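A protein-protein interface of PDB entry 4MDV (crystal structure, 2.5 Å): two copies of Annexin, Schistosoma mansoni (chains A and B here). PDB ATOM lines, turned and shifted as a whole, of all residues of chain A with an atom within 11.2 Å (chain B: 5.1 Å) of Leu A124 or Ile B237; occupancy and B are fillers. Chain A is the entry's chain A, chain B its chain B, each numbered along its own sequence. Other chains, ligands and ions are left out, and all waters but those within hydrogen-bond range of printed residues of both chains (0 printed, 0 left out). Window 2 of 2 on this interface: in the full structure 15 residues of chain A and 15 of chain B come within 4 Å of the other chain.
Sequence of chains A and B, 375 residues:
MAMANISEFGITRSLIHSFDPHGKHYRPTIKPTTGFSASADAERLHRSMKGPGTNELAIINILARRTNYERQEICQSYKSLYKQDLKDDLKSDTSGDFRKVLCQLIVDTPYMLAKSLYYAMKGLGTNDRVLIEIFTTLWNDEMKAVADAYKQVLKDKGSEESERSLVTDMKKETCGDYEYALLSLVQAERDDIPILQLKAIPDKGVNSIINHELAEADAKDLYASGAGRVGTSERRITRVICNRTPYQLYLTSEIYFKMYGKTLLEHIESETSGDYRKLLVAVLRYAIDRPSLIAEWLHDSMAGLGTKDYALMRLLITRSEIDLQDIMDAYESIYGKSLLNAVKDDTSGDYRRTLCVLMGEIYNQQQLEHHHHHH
Hydrophobic or aromatic side chains of chain A that line the printed part of chain B: Leu A124. Hydrophobic or aromatic side chains of chain B that line the printed part of chain A: Ile B237 and Tyr B276. Among the printed residues, 11 pairs touch across the chains.
The side-chain amide nitrogen (ND2) of Asn A127 sits at hydrogen-bond distance from the side-chain hydroxyl (OG) of Ser B273 (3.4 Å). The backbone NH (N) of Gly A125 is in hydrogen-bond range of the side-chain carboxylate (OD2) of Asp B177 (2.9 Å). The backbone carbonyl oxygen of Leu A124 sits at hydrogen-bond distance from the backbone NH of Ser B273, 3.1 Å away.
The side-chain hydroxyl (OG1) of Thr B238 is in hydrogen-bond range of the side-chain hydroxyl (OH) of Tyr B276 (2.5 Å). The backbone carbonyl oxygen (O) of Ala A120 sits at hydrogen-bond distance from the backbone NH (N) of Asn A127 (2.9 Å). OG1 of Thr A126 lies close to OE2 of Glu A173 (2.6 Å). The backbone carbonyl oxygen of Ile B268 sits at hydrogen-bond distance from the side-chain hydroxyl of Thr B272 (2.9 Å). ND2 of Asn A127 lies close to NH2 of Arg A129 (3.4 Å). NE of Arg B236 is in salt-bridge range of OE1 of Glu B234 (2.6 Å).
No position is printed for both chains. Of the 11 pairs that touch across the chains among the printed residues, none has its exchanged pair printed and touching as well.
No residue of chain A comes within 4 Å of Leu B222. Of chain A, only Leu A124 comes within 4 Å of Glu B234. No residue of chain A comes within 4 Å of Thr B238. No residue of chain A comes within 4 Å of Arg B239. No residue of chain A comes within 4 Å of Ile B241. No residue of chain A comes within 4 Å of Ile B268. No residue of chain A comes within 4 Å of Glu B271. Of chain A, only Leu A124 comes within 4 Å of Thr B272. Ser B273 touches just these residues of chain A: Leu A124, Gly A125, Thr A126 and Asn A127. Of the printed residues of chain B, Thr A126 touches Ser B273 (3.6 Å). Printed residues of chain A within 4 Å of Tyr B276: Leu A124 and Gly A125. Printed residues of chain A within 4 Å of Asp B177: Leu A124 (3.3 Å) and Gly A125 (2.9 Å). Of the printed residues of chain B, Gly A125 touches Asp B177, Ser B273 and Tyr B276. Printed residues of chain B within 4 Å of Asn A127: Ser B273 (3.4 Å). Leu A117 touches none of the printed residues of chain B. Tyr A119 touches none of the printed residues of chain B. The nearest printed residue of chain A that does not touch Tyr B276 is Thr A126 (5.2 Å).
Among the printed residues, merely in contact across the chains: Leu A124 with Asp B177, Leu A124 with Ile B237, Leu A124 with Glu B234, Leu A124 with Thr B272, Leu A124 with Tyr B276, Thr A126 with Ser B273, Gly A125 with Tyr B276 and Gly A125 with Ser B273.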
ATOM      1  N   LEU A 117     -28.540 -19.070  37.263  1.00  0.00           N
ATOM      2  CA  LEU A 117     -27.114 -19.409  37.190  1.00  0.00           C
ATOM      3  C   LEU A 117     -26.708 -19.502  35.729  1.00  0.00           C
ATOM      4  O   LEU A 117     -25.652 -19.016  35.317  1.00  0.00           O
ATOM      5  CB  LEU A 117     -26.825 -20.747  37.892  1.00  0.00           C
ATOM      6  CG  LEU A 117     -26.885 -20.726  39.426  1.00  0.00           C
ATOM      7  CD1 LEU A 117     -26.927 -22.149  39.963  1.00  0.00           C
ATOM      8  CD2 LEU A 117     -25.697 -19.962  40.047  1.00  0.00           C
ATOM      9  N   TYR A 118     -27.566 -20.138  34.942  1.00  0.00           N
ATOM     10  CA  TYR A 118     -27.317 -20.288  33.522  1.00  0.00           C
ATOM     11  C   TYR A 118     -27.189 -18.924  32.833  1.00  0.00           C
ATOM     12  O   TYR A 118     -26.235 -18.672  32.099  1.00  0.00           O
ATOM     13  CB  TYR A 118     -28.437 -21.108  32.899  1.00  0.00           C
ATOM     14  CG  TYR A 118     -28.458 -21.137  31.385  1.00  0.00           C
ATOM     15  CD1 TYR A 118     -27.755 -22.109  30.673  1.00  0.00           C
ATOM     16  CD2 TYR A 118     -29.209 -20.209  30.666  1.00  0.00           C
ATOM     17  CE1 TYR A 118     -27.798 -22.150  29.286  1.00  0.00           C
ATOM     18  CE2 TYR A 118     -29.250 -20.246  29.285  1.00  0.00           C
ATOM     19  CZ  TYR A 118     -28.548 -21.212  28.605  1.00  0.00           C
ATOM     20  OH  TYR A 118     -28.605 -21.235  27.242  1.00  0.00           O
ATOM     21  N   TYR A 119     -28.138 -18.030  33.078  1.00  0.00           N
ATOM     22  CA  TYR A 119     -28.049 -16.718  32.455  1.00  0.00           C
ATOM     23  C   TYR A 119     -26.899 -15.873  33.003  1.00  0.00           C
ATOM     24  O   TYR A 119     -26.372 -15.015  32.302  1.00  0.00           O
ATOM     25  CB  TYR A 119     -29.400 -15.991  32.479  1.00  0.00           C
ATOM     26  CG  TYR A 119     -30.386 -16.561  31.471  1.00  0.00           C
ATOM     27  CD1 TYR A 119     -30.082 -16.577  30.103  1.00  0.00           C
ATOM     28  CD2 TYR A 119     -31.603 -17.103  31.879  1.00  0.00           C
ATOM     29  CE1 TYR A 119     -30.968 -17.105  29.175  1.00  0.00           C
ATOM     30  CE2 TYR A 119     -32.507 -17.636  30.952  1.00  0.00           C
ATOM     31  CZ  TYR A 119     -32.185 -17.631  29.596  1.00  0.00           C
ATOM     32  OH  TYR A 119     -33.073 -18.148  28.660  1.00  0.00           O
ATOM     33  N   ALA A 120     -26.483 -16.154  34.235  1.00  0.00           N
ATOM     34  CA  ALA A 120     -25.355 -15.447  34.839  1.00  0.00           C
ATOM     35  C   ALA A 120     -24.056 -15.771  34.109  1.00  0.00           C
ATOM     36  O   ALA A 120     -23.098 -14.988  34.114  1.00  0.00           O
ATOM     37  CB  ALA A 120     -25.244 -15.797  36.303  1.00  0.00           C
ATOM     38  N   MET A 121     -24.018 -16.931  33.465  1.00  0.00           N
ATOM     39  CA  MET A 121     -22.776 -17.366  32.837  1.00  0.00           C
ATOM     40  C   MET A 121     -22.856 -17.305  31.308  1.00  0.00           C
ATOM     41  O   MET A 121     -21.882 -16.954  30.651  1.00  0.00           O
ATOM     42  CB  MET A 121     -22.388 -18.747  33.351  1.00  0.00           C
ATOM     43  CG  MET A 121     -22.212 -18.748  34.862  1.00  0.00           C
ATOM     44  SD  MET A 121     -21.518 -20.302  35.424  1.00  0.00           S
ATOM     45  CE  MET A 121     -22.942 -21.375  35.194  1.00  0.00           C
ATOM     46  N   LYS A 122     -24.024 -17.615  30.747  1.00  0.00           N
ATOM     47  CA  LYS A 122     -24.224 -17.411  29.332  1.00  0.00           C
ATOM     48  C   LYS A 122     -24.051 -15.913  29.108  1.00  0.00           C
ATOM     49  O   LYS A 122     -24.396 -15.099  29.965  1.00  0.00           O
ATOM     50  CB  LYS A 122     -25.602 -17.901  28.887  1.00  0.00           C
ATOM     51  N   GLY A 123     -23.472 -15.545  27.978  1.00  0.00           N
ATOM     52  CA  GLY A 123     -23.227 -14.141  27.722  1.00  0.00           C
ATOM     53  C   GLY A 123     -21.780 -13.749  27.930  1.00  0.00           C
ATOM     54  O   GLY A 123     -20.983 -14.523  28.451  1.00  0.00           O
ATOM     55  N   LEU A 124     -21.430 -12.541  27.505  1.00  0.00           N
ATOM     56  CA  LEU A 124     -20.068 -12.073  27.673  1.00  0.00           C
ATOM     57  C   LEU A 124     -19.866 -11.656  29.117  1.00  0.00           C
ATOM     58  O   LEU A 124     -20.722 -10.975  29.716  1.00  0.00           O
ATOM     59  CB  LEU A 124     -19.768 -10.919  26.724  1.00  0.00           C
ATOM     60  CG  LEU A 124     -19.767 -11.327  25.251  1.00  0.00           C
ATOM     61  CD1 LEU A 124     -19.796 -10.091  24.348  1.00  0.00           C
ATOM     62  CD2 LEU A 124     -18.575 -12.220  24.927  1.00  0.00           C
ATOM     63  N   GLY A 125     -18.736 -12.079  29.672  1.00  0.00           N
ATOM     64  CA  GLY A 125     -18.430 -11.803  31.057  1.00  0.00           C
ATOM     65  C   GLY A 125     -19.182 -12.767  31.942  1.00  0.00           C
ATOM     66  O   GLY A 125     -19.724 -13.768  31.484  1.00  0.00           O
ATOM     67  N   THR A 126     -19.221 -12.452  33.221  1.00  0.00           N
ATOM     68  CA  THR A 126     -19.801 -13.358  34.189  1.00  0.00           C
ATOM     69  C   THR A 126     -20.472 -12.532  35.239  1.00  0.00           C
ATOM     70  O   THR A 126     -19.845 -11.664  35.831  1.00  0.00           O
ATOM     71  CB  THR A 126     -18.731 -14.205  34.873  1.00  0.00           C
ATOM     72  OG1 THR A 126     -17.953 -14.892  33.875  1.00  0.00           O
ATOM     73  CG2 THR A 126     -19.388 -15.206  35.806  1.00  0.00           C
ATOM     74  N   ASN A 127     -21.757 -12.779  35.439  1.00  0.00           N
ATOM     75  CA  ASN A 127     -22.465 -12.127  36.513  1.00  0.00           C
ATOM     76  C   ASN A 127     -22.123 -12.751  37.856  1.00  0.00           C
ATOM     77  O   ASN A 127     -22.883 -13.548  38.408  1.00  0.00           O
ATOM     78  CB  ASN A 127     -23.943 -12.195  36.295  1.00  0.00           C
ATOM     79  CG  ASN A 127     -24.634 -11.052  36.942  1.00  0.00           C
ATOM     80  OD1 ASN A 127     -24.170 -10.550  37.970  1.00  0.00           O
ATOM     81  ND2 ASN A 127     -25.730 -10.602  36.340  1.00  0.00           N
ATOM     82  N   ASP A 128     -20.949 -12.386  38.356  1.00  0.00           N
ATOM     83  CA  ASP A 128     -20.456 -12.862  39.634  1.00  0.00           C
ATOM     84  C   ASP A 128     -21.431 -12.585  40.764  1.00  0.00           C
ATOM     85  O   ASP A 128     -21.708 -13.458  41.593  1.00  0.00           O
ATOM     86  CB  ASP A 128     -19.120 -12.199  39.915  1.00  0.00           C
ATOM     87  CG  ASP A 128     -18.030 -12.702  38.987  1.00  0.00           C
ATOM     88  OD1 ASP A 128     -17.949 -13.931  38.790  1.00  0.00           O
ATOM     89  OD2 ASP A 128     -17.265 -11.878  38.455  1.00  0.00           O
ATOM     90  N   ARG A 129     -21.968 -11.371  40.788  1.00  0.00           N
ATOM     91  CA  ARG A 129     -22.963 -11.014  41.792  1.00  0.00           C
ATOM     92  C   ARG A 129     -24.060 -12.058  41.920  1.00  0.00           C
ATOM     93  O   ARG A 129     -24.465 -12.396  43.042  1.00  0.00           O
ATOM     94  CB  ARG A 129     -23.572  -9.651  41.507  1.00  0.00           C
ATOM     95  CG  ARG A 129     -24.764  -9.307  42.388  1.00  0.00           C
ATOM     96  CD  ARG A 129     -25.399  -7.964  41.970  1.00  0.00           C
ATOM     97  NE  ARG A 129     -25.735  -7.957  40.540  1.00  0.00           N
ATOM     98  CZ  ARG A 129     -26.833  -8.505  40.008  1.00  0.00           C
ATOM     99  NH1 ARG A 129     -27.731  -9.111  40.794  1.00  0.00           N
ATOM    100  NH2 ARG A 129     -27.034  -8.450  38.684  1.00  0.00           N
ATOM    101  N   LEU A 131     -23.872 -15.345  40.918  1.00  0.00           N
ATOM    102  CA  LEU A 131     -23.294 -16.583  41.413  1.00  0.00           C
ATOM    103  C   LEU A 131     -23.104 -16.509  42.931  1.00  0.00           C
ATOM    104  O   LEU A 131     -23.403 -17.469  43.654  1.00  0.00           O
ATOM    105  CB  LEU A 131     -21.952 -16.866  40.747  1.00  0.00           C
ATOM    106  CG  LEU A 131     -21.897 -16.931  39.230  1.00  0.00           C
ATOM    107  CD1 LEU A 131     -20.449 -17.173  38.763  1.00  0.00           C
ATOM    108  CD2 LEU A 131     -22.831 -18.006  38.722  1.00  0.00           C
ATOM    109  N   LYS A 172     -15.077 -23.128  33.415  1.00  0.00           N
ATOM    110  CA  LYS A 172     -14.763 -22.355  32.214  1.00  0.00           C
ATOM    111  C   LYS A 172     -14.979 -20.869  32.475  1.00  0.00           C
ATOM    112  O   LYS A 172     -14.290 -20.011  31.916  1.00  0.00           O
ATOM    113  CB  LYS A 172     -15.615 -22.817  31.029  1.00  0.00           C
ATOM    114  N   GLU A 173     -15.928 -20.589  33.359  1.00  0.00           N
ATOM    115  CA  GLU A 173     -16.397 -19.241  33.640  1.00  0.00           C
ATOM    116  C   GLU A 173     -15.521 -18.526  34.670  1.00  0.00           C
ATOM    117  O   GLU A 173     -15.506 -17.295  34.746  1.00  0.00           O
ATOM    118  CB  GLU A 173     -17.823 -19.353  34.174  1.00  0.00           C
ATOM    119  CG  GLU A 173     -18.640 -18.113  34.033  1.00  0.00           C
ATOM    120  CD  GLU A 173     -18.881 -17.756  32.591  1.00  0.00           C
ATOM    121  OE1 GLU A 173     -18.782 -18.656  31.737  1.00  0.00           O
ATOM    122  OE2 GLU A 173     -19.161 -16.575  32.317  1.00  0.00           O
ATOM    123  N   THR A 174     -14.781 -19.311  35.447  1.00  0.00           N
ATOM    124  CA  THR A 174     -14.155 -18.787  36.655  1.00  0.00           C
ATOM    125  C   THR A 174     -12.705 -19.266  36.889  1.00  0.00           C
ATOM    126  O   THR A 174     -12.249 -20.248  36.286  1.00  0.00           O
ATOM    127  CB  THR A 174     -15.063 -19.074  37.866  1.00  0.00           C
ATOM    128  OG1 THR A 174     -14.725 -18.197  38.945  1.00  0.00           O
ATOM    129  CG2 THR A 174     -14.942 -20.530  38.294  1.00  0.00           C
ATOM    130  N   ASP B 177     -13.715 -13.445  29.387  1.00  0.00           N
ATOM    131  CA  ASP B 177     -13.784 -12.270  28.529  1.00  0.00           C
ATOM    132  C   ASP B 177     -13.005 -11.084  29.106  1.00  0.00           C
ATOM    133  O   ASP B 177     -12.298 -10.375  28.380  1.00  0.00           O
ATOM    134  CB  ASP B 177     -15.245 -11.952  28.209  1.00  0.00           C
ATOM    135  CG  ASP B 177     -15.902 -13.079  27.421  1.00  0.00           C
ATOM    136  OD1 ASP B 177     -15.188 -13.629  26.552  1.00  0.00           O
ATOM    137  OD2 ASP B 177     -17.084 -13.436  27.687  1.00  0.00           O
ATOM    138  N   LEU B 222     -21.429  -3.918  16.295  1.00  0.00           N
ATOM    139  CA  LEU B 222     -21.800  -4.099  17.700  1.00  0.00           C
ATOM    140  C   LEU B 222     -23.267  -4.465  17.865  1.00  0.00           C
ATOM    141  O   LEU B 222     -23.593  -5.386  18.613  1.00  0.00           O
ATOM    142  CB  LEU B 222     -21.464  -2.859  18.530  1.00  0.00           C
ATOM    143  CG  LEU B 222     -19.975  -2.582  18.744  1.00  0.00           C
ATOM    144  CD1 LEU B 222     -19.775  -1.382  19.659  1.00  0.00           C
ATOM    145  CD2 LEU B 222     -19.291  -3.816  19.316  1.00  0.00           C
ATOM    146  N   GLU B 234     -17.027 -13.822  22.213  1.00  0.00           N
ATOM    147  CA  GLU B 234     -17.104 -12.812  21.164  1.00  0.00           C
ATOM    148  C   GLU B 234     -16.184 -11.616  21.455  1.00  0.00           C
ATOM    149  O   GLU B 234     -16.368 -10.871  22.424  1.00  0.00           O
ATOM    150  CB  GLU B 234     -18.553 -12.372  20.958  1.00  0.00           C
ATOM    151  CG  GLU B 234     -18.805 -11.525  19.726  1.00  0.00           C
ATOM    152  CD  GLU B 234     -20.180 -10.879  19.765  1.00  0.00           C
ATOM    153  OE1 GLU B 234     -20.385  -9.834  19.104  1.00  0.00           O
ATOM    154  OE2 GLU B 234     -21.056 -11.418  20.476  1.00  0.00           O
ATOM    155  N   ARG B 235     -15.182 -11.451  20.600  1.00  0.00           N
ATOM    156  CA  ARG B 235     -14.208 -10.382  20.754  1.00  0.00           C
ATOM    157  C   ARG B 235     -14.619  -9.144  19.955  1.00  0.00           C
ATOM    158  O   ARG B 235     -13.835  -8.207  19.806  1.00  0.00           O
ATOM    159  CB  ARG B 235     -12.827 -10.857  20.307  1.00  0.00           C
ATOM    160  CG  ARG B 235     -12.691 -12.371  20.251  1.00  0.00           C
ATOM    161  CD  ARG B 235     -11.776 -12.940  21.341  1.00  0.00           C
ATOM    162  NE  ARG B 235     -12.452 -13.149  22.626  1.00  0.00           N
ATOM    163  CZ  ARG B 235     -12.008 -13.971  23.581  1.00  0.00           C
ATOM    164  NH1 ARG B 235     -10.892 -14.672  23.393  1.00  0.00           N
ATOM    165  NH2 ARG B 235     -12.678 -14.099  24.725  1.00  0.00           N
ATOM    166  N   ARG B 236     -15.849  -9.142  19.443  1.00  0.00           N
ATOM    167  CA  ARG B 236     -16.353  -8.015  18.659  1.00  0.00           C
ATOM    168  C   ARG B 236     -16.434  -6.751  19.515  1.00  0.00           C
ATOM    169  O   ARG B 236     -15.943  -5.695  19.123  1.00  0.00           O
ATOM    170  CB  ARG B 236     -17.717  -8.347  18.018  1.00  0.00           C
ATOM    171  CG  ARG B 236     -17.730  -9.647  17.193  1.00  0.00           C
ATOM    172  CD  ARG B 236     -18.788  -9.656  16.072  1.00  0.00           C
ATOM    173  NE  ARG B 236     -20.123 -10.078  16.508  1.00  0.00           N
ATOM    174  CZ  ARG B 236     -21.136 -10.343  15.678  1.00  0.00           C
ATOM    175  NH1 ARG B 236     -20.969 -10.238  14.366  1.00  0.00           N
ATOM    176  NH2 ARG B 236     -22.317 -10.721  16.159  1.00  0.00           N
ATOM    177  N   ILE B 237     -17.037  -6.866  20.695  1.00  0.00           N
ATOM    178  CA  ILE B 237     -17.157  -5.718  21.590  1.00  0.00           C
ATOM    179  C   ILE B 237     -15.788  -5.276  22.114  1.00  0.00           C
ATOM    180  O   ILE B 237     -15.471  -4.084  22.143  1.00  0.00           O
ATOM    181  CB  ILE B 237     -18.119  -6.001  22.752  1.00  0.00           C
ATOM    182  CG1 ILE B 237     -19.422  -6.591  22.202  1.00  0.00           C
ATOM    183  CG2 ILE B 237     -18.392  -4.719  23.537  1.00  0.00           C
ATOM    184  CD1 ILE B 237     -20.397  -7.052  23.260  1.00  0.00           C
ATOM    185  N   THR B 238     -14.966  -6.242  22.509  1.00  0.00           N
ATOM    186  CA  THR B 238     -13.636  -5.915  23.004  1.00  0.00           C
ATOM    187  C   THR B 238     -12.865  -5.132  21.941  1.00  0.00           C
ATOM    188  O   THR B 238     -12.338  -4.043  22.201  1.00  0.00           O
ATOM    189  CB  THR B 238     -12.825  -7.168  23.418  1.00  0.00           C
ATOM    190  OG1 THR B 238     -13.456  -7.797  24.534  1.00  0.00           O
ATOM    191  CG2 THR B 238     -11.410  -6.785  23.822  1.00  0.00           C
ATOM    192  N   ARG B 239     -12.822  -5.685  20.735  1.00  0.00           N
ATOM    193  CA  ARG B 239     -12.095  -5.060  19.645  1.00  0.00           C
ATOM    194  C   ARG B 239     -12.462  -3.589  19.474  1.00  0.00           C
ATOM    195  O   ARG B 239     -11.584  -2.751  19.289  1.00  0.00           O
ATOM    196  CB  ARG B 239     -12.328  -5.785  18.317  1.00  0.00           C
ATOM    197  CG  ARG B 239     -11.580  -5.109  17.159  1.00  0.00           C
ATOM    198  CD  ARG B 239     -12.083  -5.515  15.772  1.00  0.00           C
ATOM    199  NE  ARG B 239     -13.386  -4.939  15.440  1.00  0.00           N
ATOM    200  CZ  ARG B 239     -14.505  -5.649  15.321  1.00  0.00           C
ATOM    201  NH1 ARG B 239     -14.479  -6.965  15.504  1.00  0.00           N
ATOM    202  NH2 ARG B 239     -15.648  -5.045  15.016  1.00  0.00           N
ATOM    203  N   VAL B 240     -13.751  -3.269  19.513  1.00  0.00           N
ATOM    204  CA  VAL B 240     -14.151  -1.889  19.265  1.00  0.00           C
ATOM    205  C   VAL B 240     -13.875  -1.007  20.488  1.00  0.00           C
ATOM    206  O   VAL B 240     -13.189   0.005  20.389  1.00  0.00           O
ATOM    207  CB  VAL B 240     -15.648  -1.746  18.840  1.00  0.00           C
ATOM    208  CG1 VAL B 240     -15.940  -0.302  18.465  1.00  0.00           C
ATOM    209  CG2 VAL B 240     -16.013  -2.685  17.678  1.00  0.00           C
ATOM    210  N   ILE B 241     -14.403  -1.400  21.645  1.00  0.00           N
ATOM    211  CA  ILE B 241     -14.270  -0.578  22.839  1.00  0.00           C
ATOM    212  C   ILE B 241     -12.806  -0.375  23.207  1.00  0.00           C
ATOM    213  O   ILE B 241     -12.393   0.732  23.532  1.00  0.00           O
ATOM    214  CB  ILE B 241     -15.040  -1.161  24.055  1.00  0.00           C
ATOM    215  CG1 ILE B 241     -16.524  -1.340  23.720  1.00  0.00           C
ATOM    216  CG2 ILE B 241     -14.882  -0.244  25.260  1.00  0.00           C
ATOM    217  CD1 ILE B 241     -17.124  -0.124  23.018  1.00  0.00           C
ATOM    218  N   CYS B 242     -12.005  -1.432  23.132  1.00  0.00           N
ATOM    219  CA  CYS B 242     -10.665  -1.326  23.678  1.00  0.00           C
ATOM    220  C   CYS B 242      -9.646  -0.766  22.725  1.00  0.00           C
ATOM    221  O   CYS B 242      -8.665  -0.155  23.150  1.00  0.00           O
ATOM    222  CB  CYS B 242     -10.194  -2.661  24.228  1.00  0.00           C
ATOM    223  SG  CYS B 242     -11.137  -3.061  25.665  1.00  0.00           S
ATOM    224  N   ILE B 268     -23.912  -1.875  25.882  1.00  0.00           N
ATOM    225  CA  ILE B 268     -22.834  -2.595  26.534  1.00  0.00           C
ATOM    226  C   ILE B 268     -23.309  -3.160  27.872  1.00  0.00           C
ATOM    227  O   ILE B 268     -23.006  -4.306  28.220  1.00  0.00           O
ATOM    228  CB  ILE B 268     -21.618  -1.683  26.750  1.00  0.00           C
ATOM    229  CG1 ILE B 268     -20.845  -1.496  25.444  1.00  0.00           C
ATOM    230  CG2 ILE B 268     -20.690  -2.270  27.804  1.00  0.00           C
ATOM    231  CD1 ILE B 268     -19.793  -0.402  25.532  1.00  0.00           C
ATOM    232  N   GLU B 271     -25.668  -6.089  27.626  1.00  0.00           N
ATOM    233  CA  GLU B 271     -25.046  -7.146  26.835  1.00  0.00           C
ATOM    234  C   GLU B 271     -23.956  -7.890  27.612  1.00  0.00           C
ATOM    235  O   GLU B 271     -23.633  -9.053  27.330  1.00  0.00           O
ATOM    236  CB  GLU B 271     -24.396  -6.526  25.592  1.00  0.00           C
ATOM    237  CG  GLU B 271     -25.306  -6.303  24.411  1.00  0.00           C
ATOM    238  CD  GLU B 271     -25.532  -7.569  23.611  1.00  0.00           C
ATOM    239  OE1 GLU B 271     -26.595  -8.194  23.810  1.00  0.00           O
ATOM    240  OE2 GLU B 271     -24.649  -7.936  22.792  1.00  0.00           O
ATOM    241  N   THR B 272     -23.349  -7.200  28.564  1.00  0.00           N
ATOM    242  CA  THR B 272     -22.214  -7.784  29.263  1.00  0.00           C
ATOM    243  C   THR B 272     -22.419  -7.762  30.769  1.00  0.00           C
ATOM    244  O   THR B 272     -23.204  -6.963  31.283  1.00  0.00           O
ATOM    245  CB  THR B 272     -20.895  -7.089  28.862  1.00  0.00           C
ATOM    246  OG1 THR B 272     -20.858  -5.780  29.420  1.00  0.00           O
ATOM    247  CG2 THR B 272     -20.784  -6.983  27.336  1.00  0.00           C
ATOM    248  N   SER B 273     -21.737  -8.665  31.461  1.00  0.00           N
ATOM    249  CA  SER B 273     -21.857  -8.782  32.925  1.00  0.00           C
ATOM    250  C   SER B 273     -20.501  -8.730  33.632  1.00  0.00           C
ATOM    251  O   SER B 273     -19.456  -8.822  32.989  1.00  0.00           O
ATOM    252  CB  SER B 273     -22.603 -10.069  33.322  1.00  0.00           C
ATOM    253  OG  SER B 273     -23.995  -9.832  33.511  1.00  0.00           O
ATOM    254  N   TYR B 276     -15.960  -7.834  33.186  1.00  0.00           N
ATOM    255  CA  TYR B 276     -15.911  -7.535  31.765  1.00  0.00           C
ATOM    256  C   TYR B 276     -16.731  -6.285  31.473  1.00  0.00           C
ATOM    257  O   TYR B 276     -16.209  -5.311  30.916  1.00  0.00           O
ATOM    258  CB  TYR B 276     -16.417  -8.720  30.933  1.00  0.00           C
ATOM    259  CG  TYR B 276     -16.257  -8.522  29.443  1.00  0.00           C
ATOM    260  CD1 TYR B 276     -15.012  -8.222  28.894  1.00  0.00           C
ATOM    261  CD2 TYR B 276     -17.347  -8.627  28.585  1.00  0.00           C
ATOM    262  CE1 TYR B 276     -14.851  -8.030  27.533  1.00  0.00           C
ATOM    263  CE2 TYR B 276     -17.203  -8.438  27.233  1.00  0.00           C
ATOM    264  CZ  TYR B 276     -15.954  -8.136  26.705  1.00  0.00           C
ATOM    265  OH  TYR B 276     -15.815  -7.940  25.349  1.00  0.00           O
ATOM    266  N   LEU B 280     -15.380  -2.545  30.226  1.00  0.00           N
ATOM    267  CA  LEU B 280     -15.906  -1.955  29.000  1.00  0.00           C
ATOM    268  C   LEU B 280     -16.483  -0.589  29.319  1.00  0.00           C
ATOM    269  O   LEU B 280     -16.157   0.404  28.678  1.00  0.00           O
ATOM    270  CB  LEU B 280     -16.988  -2.844  28.382  1.00  0.00           C
ATOM    271  CG  LEU B 280     -16.631  -4.255  27.931  1.00  0.00           C
ATOM    272  CD1 LEU B 280     -17.897  -5.005  27.496  1.00  0.00           C
ATOM    273  CD2 LEU B 280     -15.564  -4.248  26.837  1.00  0.00           C
